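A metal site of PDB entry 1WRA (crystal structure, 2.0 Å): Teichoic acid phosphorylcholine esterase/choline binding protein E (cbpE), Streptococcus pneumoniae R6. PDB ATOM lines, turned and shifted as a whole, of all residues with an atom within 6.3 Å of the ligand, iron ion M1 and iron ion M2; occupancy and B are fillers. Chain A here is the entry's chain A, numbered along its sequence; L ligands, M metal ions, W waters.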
ATOM      1  N   GLY A  16      -7.384 -22.023   1.820  1.00  0.00           N
ATOM      2  CA  GLY A  16      -7.779 -21.757   3.185  1.00  0.00           C
ATOM      3  C   GLY A  16      -8.881 -20.696   3.271  1.00  0.00           C
ATOM      4  O   GLY A  16      -8.827 -19.672   2.626  1.00  0.00           O
ATOM      5  N   SER A  17      -9.920 -20.999   4.050  1.00  0.00           N
ATOM      6  CA  SER A  17     -11.076 -20.116   4.202  1.00  0.00           C
ATOM      7  C   SER A  17     -11.895 -20.610   5.392  1.00  0.00           C
ATOM      8  O   SER A  17     -11.975 -21.804   5.655  1.00  0.00           O
ATOM      9  CB  SER A  17     -11.908 -20.105   2.879  1.00  0.00           C
ATOM     10  OG  SER A  17     -13.114 -19.373   3.033  1.00  0.00           O
ATOM     11  N   ASP A  18     -12.481 -19.693   6.144  1.00  0.00           N
ATOM     12  CA  ASP A  18     -13.218 -20.060   7.347  1.00  0.00           C
ATOM     13  C   ASP A  18     -14.699 -19.740   7.152  1.00  0.00           C
ATOM     14  O   ASP A  18     -15.051 -18.589   6.926  1.00  0.00           O
ATOM     15  CB  ASP A  18     -12.787 -19.184   8.520  1.00  0.00           C
ATOM     16  CG  ASP A  18     -11.470 -19.568   9.139  1.00  0.00           C
ATOM     17  OD1 ASP A  18     -10.587 -20.139   8.500  1.00  0.00           O
ATOM     18  OD2 ASP A  18     -11.252 -19.263  10.339  1.00  0.00           O
ATOM     19  N   GLU A  35     -15.176 -17.502   1.712  1.00  0.00           N
ATOM     20  CA  GLU A  35     -14.890 -16.771   0.503  1.00  0.00           C
ATOM     21  C   GLU A  35     -16.119 -16.825  -0.427  1.00  0.00           C
ATOM     22  O   GLU A  35     -16.820 -17.854  -0.475  1.00  0.00           O
ATOM     23  CB  GLU A  35     -13.697 -17.424  -0.219  1.00  0.00           C
ATOM     24  CG  GLU A  35     -13.270 -16.737  -1.514  1.00  0.00           C
ATOM     25  CD  GLU A  35     -12.796 -15.314  -1.252  1.00  0.00           C
ATOM     26  OE1 GLU A  35     -11.661 -15.163  -0.710  1.00  0.00           O
ATOM     27  OE2 GLU A  35     -13.602 -14.368  -1.496  1.00  0.00           O
ATOM     28  N   GLY A  52      -3.420 -10.100  -6.041  1.00  0.00           N
ATOM     29  CA  GLY A  52      -3.735 -11.045  -4.979  1.00  0.00           C
ATOM     30  C   GLY A  52      -5.167 -11.042  -4.443  1.00  0.00           C
ATOM     31  O   GLY A  52      -5.541 -11.884  -3.611  1.00  0.00           O
ATOM     32  N   ILE A  53      -5.982 -10.088  -4.877  1.00  0.00           N
ATOM     33  CA  ILE A  53      -7.418 -10.175  -4.618  1.00  0.00           C
ATOM     34  C   ILE A  53      -7.893 -11.535  -5.139  1.00  0.00           C
ATOM     35  O   ILE A  53      -7.604 -11.919  -6.230  1.00  0.00           O
ATOM     36  CB  ILE A  53      -8.189  -9.043  -5.320  1.00  0.00           C
ATOM     37  CG1 ILE A  53      -7.958  -7.707  -4.564  1.00  0.00           C
ATOM     38  CG2 ILE A  53      -9.695  -9.409  -5.447  1.00  0.00           C
ATOM     39  CD1 ILE A  53      -8.683  -6.491  -5.165  1.00  0.00           C
ATOM     40  N   GLU A  54      -8.644 -12.242  -4.336  1.00  0.00           N
ATOM     41  CA  GLU A  54      -9.094 -13.544  -4.752  1.00  0.00           C
ATOM     42  C   GLU A  54     -10.250 -13.623  -5.758  1.00  0.00           C
ATOM     43  O   GLU A  54     -11.207 -12.861  -5.659  1.00  0.00           O
ATOM     44  CB  GLU A  54      -9.617 -14.297  -3.522  1.00  0.00           C
ATOM     45  CG  GLU A  54     -10.176 -15.704  -3.798  1.00  0.00           C
ATOM     46  CD  GLU A  54      -9.053 -16.629  -4.172  1.00  0.00           C
ATOM     47  OE1 GLU A  54      -8.826 -16.882  -5.381  1.00  0.00           O
ATOM     48  OE2 GLU A  54      -8.341 -17.029  -3.246  1.00  0.00           O
ATOM     49  N   HIS A  84     -12.407 -10.786  10.898  1.00  0.00           N
ATOM     50  CA  HIS A  84     -11.566  -9.760  10.283  1.00  0.00           C
ATOM     51  C   HIS A  84     -12.061  -9.595   8.842  1.00  0.00           C
ATOM     52  O   HIS A  84     -12.981 -10.333   8.441  1.00  0.00           O
ATOM     53  CB  HIS A  84     -10.046 -10.051  10.401  1.00  0.00           C
ATOM     54  CG  HIS A  84      -9.573 -11.238   9.611  1.00  0.00           C
ATOM     55  ND1 HIS A  84     -10.091 -12.490   9.781  1.00  0.00           N
ATOM     56  CD2 HIS A  84      -8.574 -11.363   8.685  1.00  0.00           C
ATOM     57  CE1 HIS A  84      -9.477 -13.331   8.970  1.00  0.00           C
ATOM     58  NE2 HIS A  84      -8.536 -12.678   8.304  1.00  0.00           N
ATOM     59  N   HIS A  86     -10.729  -9.903   5.650  1.00  0.00           N
ATOM     60  CA  HIS A  86     -10.314 -10.684   4.513  1.00  0.00           C
ATOM     61  C   HIS A  86     -11.474 -11.484   3.915  1.00  0.00           C
ATOM     62  O   HIS A  86     -12.290 -12.070   4.627  1.00  0.00           O
ATOM     63  CB  HIS A  86      -9.087 -11.572   4.825  1.00  0.00           C
ATOM     64  CG  HIS A  86      -7.899 -10.789   5.255  1.00  0.00           C
ATOM     65  ND1 HIS A  86      -6.898 -11.301   6.052  1.00  0.00           N
ATOM     66  CD2 HIS A  86      -7.555  -9.494   4.999  1.00  0.00           C
ATOM     67  CE1 HIS A  86      -5.995 -10.358   6.277  1.00  0.00           C
ATOM     68  NE2 HIS A  86      -6.363  -9.262   5.634  1.00  0.00           N
ATOM     69  N   SER A  87     -11.485 -11.479   2.600  1.00  0.00           N
ATOM     70  CA  SER A  87     -12.581 -11.998   1.780  1.00  0.00           C
ATOM     71  C   SER A  87     -12.931 -13.459   2.080  1.00  0.00           C
ATOM     72  O   SER A  87     -14.117 -13.865   1.996  1.00  0.00           O
ATOM     73  CB  SER A  87     -12.209 -11.842   0.300  1.00  0.00           C
ATOM     74  OG  SER A  87     -11.028 -12.600  -0.043  1.00  0.00           O
ATOM     75  N   ASP A  88     -11.918 -14.247   2.444  1.00  0.00           N
ATOM     76  CA  ASP A  88     -12.111 -15.669   2.779  1.00  0.00           C
ATOM     77  C   ASP A  88     -12.733 -15.899   4.180  1.00  0.00           C
ATOM     78  O   ASP A  88     -12.889 -17.045   4.643  1.00  0.00           O
ATOM     79  CB  ASP A  88     -10.790 -16.456   2.594  1.00  0.00           C
ATOM     80  CG  ASP A  88      -9.668 -15.953   3.494  1.00  0.00           C
ATOM     81  OD1 ASP A  88      -9.263 -14.759   3.368  1.00  0.00           O
ATOM     82  OD2 ASP A  88      -9.167 -16.697   4.366  1.00  0.00           O
ATOM     83  N   HIS A  89     -13.140 -14.798   4.815  1.00  0.00           N
ATOM     84  CA  HIS A  89     -13.854 -14.820   6.105  1.00  0.00           C
ATOM     85  C   HIS A  89     -15.166 -14.028   6.038  1.00  0.00           C
ATOM     86  O   HIS A  89     -16.206 -14.529   6.478  1.00  0.00           O
ATOM     87  CB  HIS A  89     -12.920 -14.313   7.247  1.00  0.00           C
ATOM     88  CG  HIS A  89     -11.650 -15.118   7.344  1.00  0.00           C
ATOM     89  ND1 HIS A  89     -11.518 -16.217   8.178  1.00  0.00           N
ATOM     90  CD2 HIS A  89     -10.502 -15.037   6.640  1.00  0.00           C
ATOM     91  CE1 HIS A  89     -10.354 -16.795   7.941  1.00  0.00           C
ATOM     92  NE2 HIS A  89      -9.700 -16.085   7.048  1.00  0.00           N
ATOM     93  N   ARG A 120      -1.356  -5.221   1.411  1.00  0.00           N
ATOM     94  CA  ARG A 120      -2.254  -6.062   2.186  1.00  0.00           C
ATOM     95  C   ARG A 120      -3.656  -5.440   2.395  1.00  0.00           C
ATOM     96  O   ARG A 120      -4.333  -5.717   3.394  1.00  0.00           O
ATOM     97  CB  ARG A 120      -1.563  -6.417   3.529  1.00  0.00           C
ATOM     98  CG  ARG A 120      -0.150  -7.041   3.374  1.00  0.00           C
ATOM     99  CD  ARG A 120       0.401  -7.783   4.627  1.00  0.00           C
ATOM    100  NE  ARG A 120       1.341  -8.857   4.240  1.00  0.00           N
ATOM    101  CZ  ARG A 120       1.088 -10.145   4.174  1.00  0.00           C
ATOM    102  NH1 ARG A 120      -0.081 -10.655   4.509  1.00  0.00           N
ATOM    103  NH2 ARG A 120       2.058 -10.950   3.796  1.00  0.00           N
ATOM    104  N   TRP A 122      -5.879  -5.465  -0.393  1.00  0.00           N
ATOM    105  CA  TRP A 122      -6.655  -6.249  -1.312  1.00  0.00           C
ATOM    106  C   TRP A 122      -8.096  -5.676  -1.504  1.00  0.00           C
ATOM    107  O   TRP A 122      -8.312  -4.519  -1.887  1.00  0.00           O
ATOM    108  CB  TRP A 122      -6.686  -7.708  -0.796  1.00  0.00           C
ATOM    109  CG  TRP A 122      -5.314  -8.319  -0.764  1.00  0.00           C
ATOM    110  CD1 TRP A 122      -4.499  -8.565  -1.839  1.00  0.00           C
ATOM    111  CD2 TRP A 122      -4.614  -8.791   0.391  1.00  0.00           C
ATOM    112  NE1 TRP A 122      -3.338  -9.167  -1.424  1.00  0.00           N
ATOM    113  CE2 TRP A 122      -3.367  -9.289  -0.053  1.00  0.00           C
ATOM    114  CE3 TRP A 122      -4.896  -8.805   1.768  1.00  0.00           C
ATOM    115  CZ2 TRP A 122      -2.411  -9.822   0.824  1.00  0.00           C
ATOM    116  CZ3 TRP A 122      -3.950  -9.330   2.640  1.00  0.00           C
ATOM    117  CH2 TRP A 122      -2.724  -9.852   2.162  1.00  0.00           C
ATOM    118  N   ASP A 123      -8.977  -6.539  -1.023  1.00  0.00           N
ATOM    119  CA  ASP A 123     -10.381  -6.667  -1.080  1.00  0.00           C
ATOM    120  C   ASP A 123     -11.092  -6.242   0.224  1.00  0.00           C
ATOM    121  O   ASP A 123     -12.323  -6.327   0.374  1.00  0.00           O
ATOM    122  CB  ASP A 123     -10.603  -8.284  -1.223  1.00  0.00           C
ATOM    123  CG  ASP A 123     -11.588  -8.470  -2.139  1.00  0.00           C
ATOM    124  OD1 ASP A 123     -11.770  -7.283  -2.585  1.00  0.00           O
ATOM    125  OD2 ASP A 123     -12.284  -9.436  -2.437  1.00  0.00           O
ATOM    126  N   ASN A 124     -10.298  -5.877   1.212  1.00  0.00           N
ATOM    127  CA  ASN A 124     -10.785  -5.814   2.585  1.00  0.00           C
ATOM    128  C   ASN A 124     -11.967  -4.821   2.728  1.00  0.00           C
ATOM    129  O   ASN A 124     -12.994  -5.138   3.278  1.00  0.00           O
ATOM    130  CB  ASN A 124      -9.684  -5.331   3.536  1.00  0.00           C
ATOM    131  CG  ASN A 124      -8.390  -6.143   3.469  1.00  0.00           C
ATOM    132  OD1 ASN A 124      -8.337  -7.234   2.876  1.00  0.00           O
ATOM    133  ND2 ASN A 124      -7.329  -5.590   4.116  1.00  0.00           N
ATOM    134  N   ASP A 180      -1.375  -6.042   9.210  1.00  0.00           N
ATOM    135  CA  ASP A 180      -2.304  -6.870   8.462  1.00  0.00           C
ATOM    136  C   ASP A 180      -3.541  -7.081   9.305  1.00  0.00           C
ATOM    137  O   ASP A 180      -3.427  -7.192  10.513  1.00  0.00           O
ATOM    138  CB  ASP A 180      -1.651  -8.237   8.185  1.00  0.00           C
ATOM    139  CG  ASP A 180      -2.499  -9.116   7.282  1.00  0.00           C
ATOM    140  OD1 ASP A 180      -3.282  -9.947   7.791  1.00  0.00           O
ATOM    141  OD2 ASP A 180      -2.440  -9.026   6.038  1.00  0.00           O
ATOM    142  N   ASP A 181      -4.711  -7.149   8.689  1.00  0.00           N
ATOM    143  CA  ASP A 181      -5.938  -7.332   9.475  1.00  0.00           C
ATOM    144  C   ASP A 181      -6.020  -8.633  10.293  1.00  0.00           C
ATOM    145  O   ASP A 181      -6.838  -8.761  11.230  1.00  0.00           O
ATOM    146  CB  ASP A 181      -7.187  -7.144   8.616  1.00  0.00           C
ATOM    147  CG  ASP A 181      -8.341  -6.507   9.372  1.00  0.00           C
ATOM    148  OD1 ASP A 181      -8.060  -5.718  10.297  1.00  0.00           O
ATOM    149  OD2 ASP A 181      -9.545  -6.758   9.114  1.00  0.00           O
ATOM    150  N   ASN A 182      -5.178  -9.610   9.948  1.00  0.00           N
ATOM    151  CA  ASN A 182      -5.094 -10.852  10.733  1.00  0.00           C
ATOM    152  C   ASN A 182      -4.880 -10.599  12.219  1.00  0.00           C
ATOM    153  O   ASN A 182      -5.484 -11.291  13.077  1.00  0.00           O
ATOM    154  CB  ASN A 182      -3.980 -11.767  10.195  1.00  0.00           C
ATOM    155  CG  ASN A 182      -4.375 -12.517   8.908  1.00  0.00           C
ATOM    156  OD1 ASN A 182      -5.479 -12.353   8.387  1.00  0.00           O
ATOM    157  ND2 ASN A 182      -3.442 -13.348   8.386  1.00  0.00           N
ATOM    158  N   SER A 185      -7.886 -10.102  14.546  1.00  0.00           N
ATOM    159  CA  SER A 185      -8.896 -11.169  14.546  1.00  0.00           C
ATOM    160  C   SER A 185      -9.683 -11.257  15.865  1.00  0.00           C
ATOM    161  O   SER A 185      -9.102 -11.324  16.962  1.00  0.00           O
ATOM    162  CB  SER A 185      -8.260 -12.534  14.269  1.00  0.00           C
ATOM    163  OG  SER A 185      -7.899 -12.664  12.913  1.00  0.00           O
ATOM    164  N   ASP A 202      -7.745 -15.545  11.940  1.00  0.00           N
ATOM    165  CA  ASP A 202      -6.360 -15.630  11.451  1.00  0.00           C
ATOM    166  C   ASP A 202      -5.394 -14.944  12.433  1.00  0.00           C
ATOM    167  O   ASP A 202      -4.353 -14.396  12.028  1.00  0.00           O
ATOM    168  CB  ASP A 202      -6.207 -14.994  10.069  1.00  0.00           C
ATOM    169  CG  ASP A 202      -6.812 -15.812   8.931  1.00  0.00           C
ATOM    170  OD1 ASP A 202      -7.318 -16.936   9.164  1.00  0.00           O
ATOM    171  OD2 ASP A 202      -6.775 -15.412   7.734  1.00  0.00           O
ATOM    172  N   HIS A 227      -5.118 -19.019  11.236  1.00  0.00           N
ATOM    173  CA  HIS A 227      -4.629 -18.688   9.916  1.00  0.00           C
ATOM    174  C   HIS A 227      -4.340 -19.943   9.061  1.00  0.00           C
ATOM    175  O   HIS A 227      -3.300 -20.008   8.387  1.00  0.00           O
ATOM    176  CB  HIS A 227      -3.412 -17.760  10.017  1.00  0.00           C
ATOM    177  CG  HIS A 227      -3.048 -17.063   8.729  1.00  0.00           C
ATOM    178  ND1 HIS A 227      -1.837 -16.450   8.534  1.00  0.00           N
ATOM    179  CD2 HIS A 227      -3.741 -16.916   7.574  1.00  0.00           C
ATOM    180  CE1 HIS A 227      -1.806 -15.922   7.313  1.00  0.00           C
ATOM    181  NE2 HIS A 227      -2.930 -16.211   6.705  1.00  0.00           N
ATOM    182  N   HIS A 228      -5.276 -20.891   9.117  1.00  0.00           N
ATOM    183  CA  HIS A 228      -5.401 -22.025   8.185  1.00  0.00           C
ATOM    184  C   HIS A 228      -4.307 -23.131   8.326  1.00  0.00           C
ATOM    185  O   HIS A 228      -4.624 -24.314   8.586  1.00  0.00           O
ATOM    186  CB  HIS A 228      -5.424 -21.485   6.758  1.00  0.00           C
ATOM    187  CG  HIS A 228      -6.464 -20.420   6.518  1.00  0.00           C
ATOM    188  ND1 HIS A 228      -7.807 -20.694   6.457  1.00  0.00           N
ATOM    189  CD2 HIS A 228      -6.337 -19.089   6.317  1.00  0.00           C
ATOM    190  CE1 HIS A 228      -8.473 -19.578   6.233  1.00  0.00           C
ATOM    191  NE2 HIS A 228      -7.607 -18.587   6.153  1.00  0.00           N
HETATM  192  P1  LIG L   1      -4.909 -14.913   4.822  1.00  0.00           P
HETATM  193  O1  LIG L   1      -5.865 -16.212   5.058  1.00  0.00           O
HETATM  194  O2  LIG L   1      -3.531 -15.428   4.457  1.00  0.00           O
HETATM  195  O3  LIG L   1      -4.848 -13.808   5.922  1.00  0.00           O
HETATM  196  O4  LIG L   1      -5.545 -14.113   3.541  1.00  0.00           O
HETATM  197  C1  LIG L   1      -5.074 -14.290   2.219  1.00  0.00           C
HETATM  198  C2  LIG L   1      -5.164 -13.010   1.388  1.00  0.00           C
HETATM  199  N1  LIG L   1      -6.494 -12.638   0.779  1.00  0.00           N
HETATM  200  C3  LIG L   1      -7.439 -13.790   0.686  1.00  0.00           C
HETATM  201  C4  LIG L   1      -7.186 -11.559   1.554  1.00  0.00           C
HETATM  202  C5  LIG L   1      -6.204 -12.098  -0.589  1.00  0.00           C
HETATM  203 FE    FE M   1      -6.692 -13.295   6.948  1.00  0.00          FE
HETATM  204 FE    FE M   2      -7.830 -16.367   6.060  1.00  0.00          FE
HETATM  205  O   HOH W   1      -7.699 -14.312   5.413  1.00  0.00           O
HETATM  206  O   HOH W   2      -9.656  -9.485   1.487  1.00  0.00           O
HETATM  207  O   HOH W   3      -6.517 -18.035   2.834  1.00  0.00           O
HETATM  208  O   HOH W   4      -9.377 -11.299  -1.641  1.00  0.00           O
HETATM  209  O   HOH W   5      -2.727 -11.903   5.438  1.00  0.00           O
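Iron ion M1 is bound by water W1 (2.1 Å), the side-chain amide oxygen of Asn 182 (2.1 Å), an oxygen (O3) of the ligand (2.2 Å), a ring nitrogen (ND1) of His 86 (2.2 Å), the side-chain carboxylate of Asp 202 (2.3 Å) and a ring nitrogen (NE2) of His 84 (2.4 Å).
Iron ion M2 is bound by a ring nitrogen (NE2) of His 89 (2.1 Å), water W1 (2.2 Å), the side-chain carboxylate (OD2) of Asp 88 (2.2 Å), the side-chain carboxylate (OD2) of Asp 202 (2.2 Å), an oxygen (O1) of the ligand (2.2 Å) and a ring nitrogen (NE2) of His 228 (2.2 Å). Iron ion M2 has six donor atoms within binding distance.
A ring nitrogen (NE2) of His 227 sits at hydrogen-bond distance from an oxygen (O2) of the ligand (2.5 Å).
Water W1 bridges the side-chain carboxylate (OD1) of Asp 88 (2.6 Å) and an oxygen (O4) of the ligand (2.9 Å). Water W5 lies within hydrogen-bond range of the side-chain carboxylate (OD2) of Asp 180, the guanidinium group (NH1) of Arg 120 and the side-chain amide nitrogen (ND2) of Asn 182. Water W2 bridges N of Ser 87 (2.9 Å) and OD1 of Asn 124 (3.0 Å). Water W4 bridges OG of Ser 87 (2.6 Å) and N of Glu 54 (2.9 Å).
Within 4 Å of iron ion M1: His 84, His 86, Asn 182 and Asp 202. Along chain A the residues within 4 Å of iron ion M1 span positions 84 to 202.
N of Asn 182 is in hydrogen-bond range of OD1 of Asp 180 (2.9 Å). OE1 of Glu 35 lies within hydrogen-bond range of N of Asp 88. The backbone carbonyl oxygen (O) of Asp 88 lies within hydrogen-bond range of the backbone NH (N) of Asp 18 (3.1 Å). The side-chain hydroxyl (OG) of Ser 17 is in hydrogen-bond range of the backbone carbonyl oxygen (O) of Asp 88. The backbone NH (N) of Asp 202 lies within hydrogen-bond range of the side-chain hydroxyl (OG) of Ser 185, 3.0 Å away. ND1 of His 228 lies close to OD1 of Asp 18. ND1 of His 228 lies close to N of Ser 17 (3.2 Å). The side-chain carboxylate of Glu 35 sits at hydrogen-bond distance from the side-chain hydroxyl of Ser 87 (2.7 Å).
Merely in contact with the ligand: Gly 52 (3.1 Å), Ser 87 (3.9 Å) and Trp 122 (3.6 Å). Within 4 Å of the ligand: Gly 52, His 86, Ser 87, Asp 88, Trp 122, Asn 182, Asp 202, His 227 and His 228. The nearest printed residue that does not touch the ligand is His 89 (4.3 Å).
Four residues have an atom within 4 Å of iron ion M2: Asp 88, His 89, Asp 202 and His 228. The nearest printed residue that does not touch iron ion M2 is His 84 (4.4 Å).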
